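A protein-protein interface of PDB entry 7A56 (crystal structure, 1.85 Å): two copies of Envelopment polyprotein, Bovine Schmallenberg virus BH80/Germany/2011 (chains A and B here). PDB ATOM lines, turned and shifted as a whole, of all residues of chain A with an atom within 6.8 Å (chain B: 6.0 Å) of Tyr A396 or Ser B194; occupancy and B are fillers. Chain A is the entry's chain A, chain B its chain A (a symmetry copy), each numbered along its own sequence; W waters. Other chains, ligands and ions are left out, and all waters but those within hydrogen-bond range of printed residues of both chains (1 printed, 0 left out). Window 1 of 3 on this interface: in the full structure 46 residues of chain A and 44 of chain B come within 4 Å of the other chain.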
ATOM      1  N   GLU A 311       2.305  10.831  -9.347  1.00  0.00           N
ATOM      2  CA  GLU A 311       2.966   9.563  -9.682  1.00  0.00           C
ATOM      3  C   GLU A 311       2.495   9.022 -11.020  1.00  0.00           C
ATOM      4  O   GLU A 311       1.294   9.001 -11.322  1.00  0.00           O
ATOM      5  CB  GLU A 311       2.704   8.532  -8.596  1.00  0.00           C
ATOM      6  CG  GLU A 311       3.263   8.969  -7.256  1.00  0.00           C
ATOM      7  CD  GLU A 311       3.355   7.824  -6.263  1.00  0.00           C
ATOM      8  OE1 GLU A 311       2.637   6.814  -6.465  1.00  0.00           O
ATOM      9  OE2 GLU A 311       4.164   7.943  -5.303  1.00  0.00           O
ATOM     10  N   GLN A 312       3.441   8.608 -11.838  1.00  0.00           N
ATOM     11  CA  GLN A 312       3.062   8.017 -13.092  1.00  0.00           C
ATOM     12  C   GLN A 312       2.591   6.607 -12.759  1.00  0.00           C
ATOM     13  O   GLN A 312       3.165   5.956 -11.886  1.00  0.00           O
ATOM     14  CB  GLN A 312       4.244   7.978 -14.049  1.00  0.00           C
ATOM     15  CG  GLN A 312       3.828   7.417 -15.385  1.00  0.00           C
ATOM     16  CD  GLN A 312       4.967   6.788 -16.126  1.00  0.00           C
ATOM     17  OE1 GLN A 312       6.128   6.944 -15.747  1.00  0.00           O
ATOM     18  NE2 GLN A 312       4.652   6.087 -17.200  1.00  0.00           N
ATOM     19  N   ASP A 313       1.516   6.174 -13.388  1.00  0.00           N
ATOM     20  CA  ASP A 313       1.006   4.808 -13.221  1.00  0.00           C
ATOM     21  C   ASP A 313       1.352   4.049 -14.499  1.00  0.00           C
ATOM     22  O   ASP A 313       0.680   4.179 -15.531  1.00  0.00           O
ATOM     23  CB  ASP A 313      -0.488   4.844 -12.875  1.00  0.00           C
ATOM     24  CG  ASP A 313      -1.070   3.443 -12.591  1.00  0.00           C
ATOM     25  OD1 ASP A 313      -0.416   2.443 -12.921  1.00  0.00           O
ATOM     26  OD2 ASP A 313      -2.190   3.329 -12.065  1.00  0.00           O
ATOM     27  N   ASN A 314       2.408   3.233 -14.427  1.00  0.00           N
ATOM     28  CA  ASN A 314       2.854   2.450 -15.574  1.00  0.00           C
ATOM     29  C   ASN A 314       1.853   1.392 -16.010  1.00  0.00           C
ATOM     30  O   ASN A 314       1.974   0.910 -17.135  1.00  0.00           O
ATOM     31  CB  ASN A 314       4.178   1.758 -15.292  1.00  0.00           C
ATOM     32  CG  ASN A 314       5.324   2.671 -15.507  1.00  0.00           C
ATOM     33  OD1 ASN A 314       6.050   3.003 -14.576  1.00  0.00           O
ATOM     34  ND2 ASN A 314       5.469   3.145 -16.740  1.00  0.00           N
ATOM     35  N   THR A 315       0.847   1.067 -15.196  1.00  0.00           N
ATOM     36  CA  THR A 315      -0.143   0.096 -15.668  1.00  0.00           C
ATOM     37  C   THR A 315      -1.129   0.722 -16.631  1.00  0.00           C
ATOM     38  O   THR A 315      -1.854  -0.006 -17.317  1.00  0.00           O
ATOM     39  CB  THR A 315      -0.895  -0.523 -14.494  1.00  0.00           C
ATOM     40  OG1 THR A 315      -1.784   0.435 -13.889  1.00  0.00           O
ATOM     41  CG2 THR A 315       0.109  -1.130 -13.443  1.00  0.00           C
ATOM     42  N   CYS A 369      10.501   9.354  -4.612  1.00  0.00           N
ATOM     43  CA  CYS A 369      10.341  10.225  -5.758  1.00  0.00           C
ATOM     44  C   CYS A 369       9.062   9.899  -6.504  1.00  0.00           C
ATOM     45  O   CYS A 369       8.493   8.820  -6.332  1.00  0.00           O
ATOM     46  CB  CYS A 369      11.552  10.080  -6.671  1.00  0.00           C
ATOM     47  SG  CYS A 369      12.980  10.729  -5.823  1.00  0.00           S
ATOM     48  N   PRO A 370       8.570  10.821  -7.336  1.00  0.00           N
ATOM     49  CA  PRO A 370       7.355  10.503  -8.103  1.00  0.00           C
ATOM     50  C   PRO A 370       7.533   9.267  -8.959  1.00  0.00           C
ATOM     51  O   PRO A 370       6.693   8.353  -8.907  1.00  0.00           O
ATOM     52  CB  PRO A 370       7.122  11.764  -8.947  1.00  0.00           C
ATOM     53  CG  PRO A 370       7.941  12.847  -8.297  1.00  0.00           C
ATOM     54  CD  PRO A 370       9.101  12.161  -7.664  1.00  0.00           C
ATOM     55  N   GLU A 371       8.619   9.197  -9.737  1.00  0.00           N
ATOM     56  CA  GLU A 371       8.857   8.036 -10.597  1.00  0.00           C
ATOM     57  C   GLU A 371       9.540   6.895  -9.859  1.00  0.00           C
ATOM     58  O   GLU A 371       9.791   5.846 -10.466  1.00  0.00           O
ATOM     59  CB  GLU A 371       9.689   8.422 -11.827  1.00  0.00           C
ATOM     60  CG  GLU A 371       9.058   9.504 -12.695  1.00  0.00           C
ATOM     61  CD  GLU A 371       8.703   9.013 -14.091  1.00  0.00           C
ATOM     62  OE1 GLU A 371       8.041   9.781 -14.829  1.00  0.00           O
ATOM     63  OE2 GLU A 371       9.087   7.872 -14.446  1.00  0.00           O
ATOM     64  N   GLY A 372       9.842   7.090  -8.576  1.00  0.00           N
ATOM     65  CA  GLY A 372      10.519   6.071  -7.802  1.00  0.00           C
ATOM     66  C   GLY A 372      11.820   5.716  -8.472  1.00  0.00           C
ATOM     67  O   GLY A 372      12.591   6.587  -8.887  1.00  0.00           O
ATOM     68  N   ASP A 394      10.157  -2.614  -3.425  1.00  0.00           N
ATOM     69  CA  ASP A 394       8.726  -2.796  -3.628  1.00  0.00           C
ATOM     70  C   ASP A 394       8.383  -2.625  -5.107  1.00  0.00           C
ATOM     71  O   ASP A 394       9.037  -1.872  -5.823  1.00  0.00           O
ATOM     72  CB  ASP A 394       7.950  -1.796  -2.787  1.00  0.00           C
ATOM     73  CG  ASP A 394       8.008  -2.118  -1.322  1.00  0.00           C
ATOM     74  OD1 ASP A 394       7.701  -3.270  -0.951  1.00  0.00           O
ATOM     75  OD2 ASP A 394       8.346  -1.219  -0.533  1.00  0.00           O
ATOM     76  N   THR A 395       7.356  -3.342  -5.571  1.00  0.00           N
ATOM     77  CA  THR A 395       6.963  -3.326  -6.982  1.00  0.00           C
ATOM     78  C   THR A 395       5.541  -2.797  -7.106  1.00  0.00           C
ATOM     79  O   THR A 395       4.791  -2.735  -6.138  1.00  0.00           O
ATOM     80  CB  THR A 395       7.054  -4.722  -7.636  1.00  0.00           C
ATOM     81  OG1 THR A 395       6.108  -5.597  -7.014  1.00  0.00           O
ATOM     82  CG2 THR A 395       8.416  -5.311  -7.420  1.00  0.00           C
ATOM     83  N   TYR A 396       5.170  -2.425  -8.318  1.00  0.00           N
ATOM     84  CA  TYR A 396       3.837  -1.909  -8.596  1.00  0.00           C
ATOM     85  C   TYR A 396       3.048  -2.859  -9.492  1.00  0.00           C
ATOM     86  O   TYR A 396       1.925  -2.541  -9.903  1.00  0.00           O
ATOM     87  CB  TYR A 396       3.932  -0.505  -9.222  1.00  0.00           C
ATOM     88  CG  TYR A 396       4.264   0.580  -8.197  1.00  0.00           C
ATOM     89  CD1 TYR A 396       5.597   0.868  -7.847  1.00  0.00           C
ATOM     90  CD2 TYR A 396       3.259   1.350  -7.608  1.00  0.00           C
ATOM     91  CE1 TYR A 396       5.897   1.835  -6.933  1.00  0.00           C
ATOM     92  CE2 TYR A 396       3.564   2.356  -6.701  1.00  0.00           C
ATOM     93  CZ  TYR A 396       4.884   2.590  -6.367  1.00  0.00           C
ATOM     94  OH  TYR A 396       5.224   3.546  -5.467  1.00  0.00           O
ATOM     95  N   ILE A 397       3.606  -4.036  -9.750  1.00  0.00           N
ATOM     96  CA  ILE A 397       2.918  -5.166 -10.365  1.00  0.00           C
ATOM     97  C   ILE A 397       3.442  -6.410  -9.673  1.00  0.00           C
ATOM     98  O   ILE A 397       4.607  -6.458  -9.246  1.00  0.00           O
ATOM     99  CB  ILE A 397       3.140  -5.309 -11.900  1.00  0.00           C
ATOM    100  CG1 ILE A 397       4.652  -5.409 -12.216  1.00  0.00           C
ATOM    101  CG2 ILE A 397       2.398  -4.162 -12.638  1.00  0.00           C
ATOM    102  CD1 ILE A 397       4.990  -5.590 -13.669  1.00  0.00           C
ATOM    103  N   LYS A 398       2.591  -7.453  -9.622  1.00  0.00           N
ATOM    104  CA  LYS A 398       3.033  -8.757  -9.105  1.00  0.00           C
ATOM    105  C   LYS A 398       3.296  -9.775 -10.205  1.00  0.00           C
ATOM    106  O   LYS A 398       4.105 -10.678 -10.009  1.00  0.00           O
ATOM    107  CB  LYS A 398       1.991  -9.345  -8.124  1.00  0.00           C
ATOM    108  CG  LYS A 398       1.659  -8.466  -6.922  1.00  0.00           C
ATOM    109  CD  LYS A 398       2.931  -8.244  -6.069  1.00  0.00           C
ATOM    110  CE  LYS A 398       3.538  -9.558  -5.513  1.00  0.00           C
ATOM    111  NZ  LYS A 398       4.755  -9.276  -4.629  1.00  0.00           N
ATOM    112  N   ILE A 411       9.453  -1.143 -15.592  1.00  0.00           N
ATOM    113  CA  ILE A 411       8.753  -1.285 -14.318  1.00  0.00           C
ATOM    114  C   ILE A 411       9.163  -0.140 -13.406  1.00  0.00           C
ATOM    115  O   ILE A 411      10.226   0.461 -13.566  1.00  0.00           O
ATOM    116  CB  ILE A 411       9.062  -2.614 -13.595  1.00  0.00           C
ATOM    117  CG1 ILE A 411      10.524  -2.702 -13.169  1.00  0.00           C
ATOM    118  CG2 ILE A 411       8.589  -3.812 -14.420  1.00  0.00           C
ATOM    119  CD1 ILE A 411      10.883  -4.088 -12.637  1.00  0.00           C
ATOM    120  N   LYS A 412       8.311   0.142 -12.423  1.00  0.00           N
ATOM    121  CA  LYS A 412       8.612   1.146 -11.411  1.00  0.00           C
ATOM    122  C   LYS A 412       8.771   0.453 -10.064  1.00  0.00           C
ATOM    123  O   LYS A 412       8.037  -0.496  -9.757  1.00  0.00           O
ATOM    124  CB  LYS A 412       7.518   2.213 -11.371  1.00  0.00           C
ATOM    125  CG  LYS A 412       7.603   3.170 -10.211  1.00  0.00           C
ATOM    126  CD  LYS A 412       6.530   4.254 -10.311  1.00  0.00           C
ATOM    127  CE  LYS A 412       5.113   3.749  -9.987  1.00  0.00           C
ATOM    128  NZ  LYS A 412       4.153   4.881  -9.657  1.00  0.00           N
ATOM    129  N   LEU A 413       9.788   0.870  -9.311  1.00  0.00           N
ATOM    130  CA  LEU A 413      10.142   0.294  -8.020  1.00  0.00           C
ATOM    131  C   LEU A 413      10.161   1.360  -6.937  1.00  0.00           C
ATOM    132  O   LEU A 413      10.440   2.536  -7.183  1.00  0.00           O
ATOM    133  CB  LEU A 413      11.516  -0.386  -8.056  1.00  0.00           C
ATOM    134  CG  LEU A 413      11.680  -1.505  -9.091  1.00  0.00           C
ATOM    135  CD1 LEU A 413      13.115  -2.013  -9.014  1.00  0.00           C
ATOM    136  CD2 LEU A 413      10.653  -2.630  -8.924  1.00  0.00           C
ATOM    137  N   ASN A 414       9.882   0.928  -5.733  1.00  0.00           N
ATOM    138  CA  ASN A 414       9.981   1.779  -4.562  1.00  0.00           C
ATOM    139  C   ASN A 414      11.089   1.173  -3.722  1.00  0.00           C
ATOM    140  O   ASN A 414      10.864   0.170  -3.042  1.00  0.00           O
ATOM    141  CB  ASN A 414       8.655   1.834  -3.811  1.00  0.00           C
ATOM    142  CG  ASN A 414       8.773   2.502  -2.462  1.00  0.00           C
ATOM    143  OD1 ASN A 414       8.663   1.854  -1.406  1.00  0.00           O
ATOM    144  ND2 ASN A 414       8.978   3.810  -2.480  1.00  0.00           N
ATOM    145  N   LYS B 112      -2.095  -6.634   1.850  1.00  0.00           N
ATOM    146  CA  LYS B 112      -1.049  -5.788   2.439  1.00  0.00           C
ATOM    147  C   LYS B 112      -0.449  -4.917   1.359  1.00  0.00           C
ATOM    148  O   LYS B 112      -0.466  -5.277   0.173  1.00  0.00           O
ATOM    149  CB  LYS B 112       0.070  -6.614   3.099  1.00  0.00           C
ATOM    150  CG  LYS B 112       0.841  -7.486   2.169  1.00  0.00           C
ATOM    151  CD  LYS B 112       1.847  -8.384   2.954  1.00  0.00           C
ATOM    152  CE  LYS B 112       2.547  -9.394   2.026  1.00  0.00           C
ATOM    153  NZ  LYS B 112       3.407 -10.398   2.747  1.00  0.00           N
ATOM    154  N   ALA B 113       0.083  -3.758   1.775  1.00  0.00           N
ATOM    155  CA  ALA B 113       0.892  -2.947   0.869  1.00  0.00           C
ATOM    156  C   ALA B 113       1.905  -2.139   1.702  1.00  0.00           C
ATOM    157  O   ALA B 113       1.771  -1.986   2.930  1.00  0.00           O
ATOM    158  CB  ALA B 113       0.014  -2.022   0.002  1.00  0.00           C
ATOM    159  N   SER B 114       2.970  -1.710   1.023  1.00  0.00           N
ATOM    160  CA  SER B 114       3.961  -0.839   1.618  1.00  0.00           C
ATOM    161  C   SER B 114       3.461   0.602   1.563  1.00  0.00           C
ATOM    162  O   SER B 114       2.696   0.993   0.673  1.00  0.00           O
ATOM    163  CB  SER B 114       5.311  -0.930   0.881  1.00  0.00           C
ATOM    164  OG  SER B 114       5.658  -2.318   0.689  1.00  0.00           O
ATOM    165  N   TYR B 115       3.912   1.397   2.528  1.00  0.00           N
ATOM    166  CA  TYR B 115       3.608   2.828   2.580  1.00  0.00           C
ATOM    167  C   TYR B 115       4.882   3.590   2.883  1.00  0.00           C
ATOM    168  O   TYR B 115       5.814   3.064   3.514  1.00  0.00           O
ATOM    169  CB  TYR B 115       2.537   3.145   3.653  1.00  0.00           C
ATOM    170  CG  TYR B 115       1.134   2.692   3.258  1.00  0.00           C
ATOM    171  CD1 TYR B 115       0.807   1.305   3.151  1.00  0.00           C
ATOM    172  CD2 TYR B 115       0.134   3.625   2.982  1.00  0.00           C
ATOM    173  CE1 TYR B 115      -0.477   0.921   2.765  1.00  0.00           C
ATOM    174  CE2 TYR B 115      -1.133   3.267   2.624  1.00  0.00           C
ATOM    175  CZ  TYR B 115      -1.442   1.872   2.513  1.00  0.00           C
ATOM    176  OH  TYR B 115      -2.700   1.481   2.111  1.00  0.00           O
ATOM    177  N   ARG B 116       4.889   4.869   2.471  1.00  0.00           N
ATOM    178  CA  ARG B 116       6.038   5.724   2.731  1.00  0.00           C
ATOM    179  C   ARG B 116       5.628   7.044   3.382  1.00  0.00           C
ATOM    180  O   ARG B 116       4.568   7.634   3.116  1.00  0.00           O
ATOM    181  CB  ARG B 116       6.865   6.029   1.477  1.00  0.00           C
ATOM    182  CG  ARG B 116       6.132   6.734   0.417  1.00  0.00           C
ATOM    183  CD  ARG B 116       7.099   7.173  -0.689  1.00  0.00           C
ATOM    184  NE  ARG B 116       6.355   7.732  -1.817  1.00  0.00           N
ATOM    185  CZ  ARG B 116       6.205   9.031  -2.049  1.00  0.00           C
ATOM    186  NH1 ARG B 116       5.499   9.448  -3.100  1.00  0.00           N
ATOM    187  NH2 ARG B 116       6.783   9.921  -1.248  1.00  0.00           N
ATOM    188  N   LYS B 192       0.590   5.129  -0.085  1.00  0.00           N
ATOM    189  CA  LYS B 192       0.835   3.743  -0.585  1.00  0.00           C
ATOM    190  C   LYS B 192       1.967   3.764  -1.615  1.00  0.00           C
ATOM    191  O   LYS B 192       1.989   4.628  -2.505  1.00  0.00           O
ATOM    192  CB  LYS B 192      -0.461   3.212  -1.198  1.00  0.00           C
ATOM    193  CG  LYS B 192      -0.395   1.719  -1.700  1.00  0.00           C
ATOM    194  CD  LYS B 192      -1.814   1.118  -1.807  1.00  0.00           C
ATOM    195  CE  LYS B 192      -2.600   1.801  -2.883  1.00  0.00           C
ATOM    196  NZ  LYS B 192      -4.076   1.546  -2.751  1.00  0.00           N
ATOM    197  N   SER B 193       2.961   2.864  -1.446  1.00  0.00           N
ATOM    198  CA  SER B 193       4.188   2.874  -2.241  1.00  0.00           C
ATOM    199  C   SER B 193       4.492   1.501  -2.844  1.00  0.00           C
ATOM    200  O   SER B 193       5.662   1.179  -3.092  1.00  0.00           O
ATOM    201  CB  SER B 193       5.372   3.374  -1.397  1.00  0.00           C
ATOM    202  OG  SER B 193       5.607   2.536  -0.253  1.00  0.00           O
ATOM    203  N   SER B 194       3.453   0.688  -3.077  1.00  0.00           N
ATOM    204  CA  SER B 194       3.553  -0.596  -3.776  1.00  0.00           C
ATOM    205  C   SER B 194       2.163  -0.925  -4.310  1.00  0.00           C
ATOM    206  O   SER B 194       1.165  -0.286  -3.946  1.00  0.00           O
ATOM    207  CB  SER B 194       4.043  -1.724  -2.861  1.00  0.00           C
ATOM    208  OG  SER B 194       3.027  -2.067  -1.932  1.00  0.00           O
ATOM    209  N   ILE B 195       2.095  -1.913  -5.191  1.00  0.00           N
ATOM    210  CA  ILE B 195       0.793  -2.527  -5.424  1.00  0.00           C
ATOM    211  C   ILE B 195       0.362  -3.247  -4.142  1.00  0.00           C
ATOM    212  O   ILE B 195       1.190  -3.630  -3.290  1.00  0.00           O
ATOM    213  CB  ILE B 195       0.876  -3.487  -6.629  1.00  0.00           C
ATOM    214  CG1 ILE B 195      -0.525  -3.941  -7.088  1.00  0.00           C
ATOM    215  CG2 ILE B 195       1.834  -4.630  -6.298  1.00  0.00           C
ATOM    216  CD1 ILE B 195      -0.565  -4.614  -8.509  1.00  0.00           C
ATOM    217  N   GLU B 196      -0.938  -3.395  -3.954  1.00  0.00           N
ATOM    218  CA  GLU B 196      -1.296  -4.241  -2.835  1.00  0.00           C
ATOM    219  C   GLU B 196      -1.245  -5.688  -3.305  1.00  0.00           C
ATOM    220  O   GLU B 196      -1.280  -5.955  -4.503  1.00  0.00           O
ATOM    221  CB  GLU B 196      -2.691  -3.905  -2.290  1.00  0.00           C
ATOM    222  CG  GLU B 196      -3.887  -4.226  -3.234  1.00  0.00           C
ATOM    223  CD  GLU B 196      -5.235  -3.982  -2.527  1.00  0.00           C
ATOM    224  OE1 GLU B 196      -5.587  -2.809  -2.321  1.00  0.00           O
ATOM    225  OE2 GLU B 196      -5.951  -4.941  -2.152  1.00  0.00           O
ATOM    226  N   GLN B 197      -1.084  -6.603  -2.365  1.00  0.00           N
ATOM    227  CA  GLN B 197      -1.040  -8.026  -2.728  1.00  0.00           C
ATOM    228  C   GLN B 197      -1.786  -8.833  -1.684  1.00  0.00           C
ATOM    229  O   GLN B 197      -1.903  -8.428  -0.524  1.00  0.00           O
ATOM    230  CB  GLN B 197       0.419  -8.507  -2.885  1.00  0.00           C
ATOM    231  CG  GLN B 197       1.249  -8.418  -1.619  1.00  0.00           C
ATOM    232  CD  GLN B 197       2.693  -8.705  -1.928  1.00  0.00           C
ATOM    233  OE1 GLN B 197       3.357  -7.891  -2.581  1.00  0.00           O
ATOM    234  NE2 GLN B 197       3.185  -9.879  -1.513  1.00  0.00           N
HETATM  235  O   HOH W   1       8.187   2.360   1.557  1.00  0.00           O
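Water W1 lies within hydrogen-bond range of the side-chain amide oxygen (OD1) of Asn A414 (3.0 Å), the backbone carbonyl oxygen (O) of Tyr B115 (3.2 Å) and the side-chain hydroxyl (OG) of Ser B193 (3.2 Å).
N of Asp A394 is in hydrogen-bond range of O of Asn A414 (2.9 Å).
O of Ile A397 is in hydrogen-bond range of OG1 of Thr A395 (2.8 Å).
N of Gln B197 sits at hydrogen-bond distance from O of Lys B112.
The backbone NH of Ser B193 is in hydrogen-bond range of the backbone carbonyl oxygen of Ser B114 (2.8 Å).
The side-chain hydroxyl of Ser B194 is in hydrogen-bond range of the backbone NH of Ser B114 (3.0 Å).
OG of Ser B193 lies close to N of Tyr B115, at 3.5 Å.
Among the printed residues, pairs that only touch across the chains: Asp A394 with Ser B193, Asp A394 with Ser B194, Thr A395 with Ser B194, Tyr A396 with Ser B194, Tyr A396 with Ile B195, Ile A397 with Ile B195 and Lys A398 with Ile B195.
Of the 11 printed residues of chain B, 6 touch a printed residue of chain A.
Hydrophobic or aromatic side chains of chain A within 4 Å of the printed part of chain B: Tyr A396.
Among the printed residues, Asp or Glu carboxylates within 4 Å of a Lys or Arg side-chain nitrogen of the other chain: Glu A311 with Arg B116.
Of the printed residues of chain B, Tyr A396 touches Ser B193, Ser B194 and Ile B195.
Printed residues of chain A within 4 Å of Ser B194: Asp A394, Thr A395 and Tyr A396.
Of the printed residues of chain A, Ser B114 touches Asp A394 (2.8 Å).
Of the printed residues of chain A, Arg B116 touches Glu A311.
Of the printed residues of chain B, Thr A395 touches Ser B194 (3.4 Å) and Ile B195 (3.0 Å).
Asp A313 touches none of the printed residues of chain B.
No position is printed for both chains.
The side-chain carboxylate (OE2) of Glu A311 is in salt-bridge range of the guanidinium group (NH1) of Arg B116.
The side-chain carboxylate of Asp A394 sits at hydrogen-bond distance from the side-chain hydroxyl of Ser B114.
O of Thr A395 sits at hydrogen-bond distance from N of Ile B195 (3.0 Å).
The backbone carbonyl oxygen of Ser B193 sits at hydrogen-bond distance from the side-chain hydroxyl of Tyr A396 (3.4 Å).
The side-chain amino group (NZ) of Lys A398 sits at hydrogen-bond distance from the side-chain amide oxygen (OE1) of Gln B197 (2.8 Å).
OD1 of Asn A414 sits at hydrogen-bond distance from OG of Ser B193.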
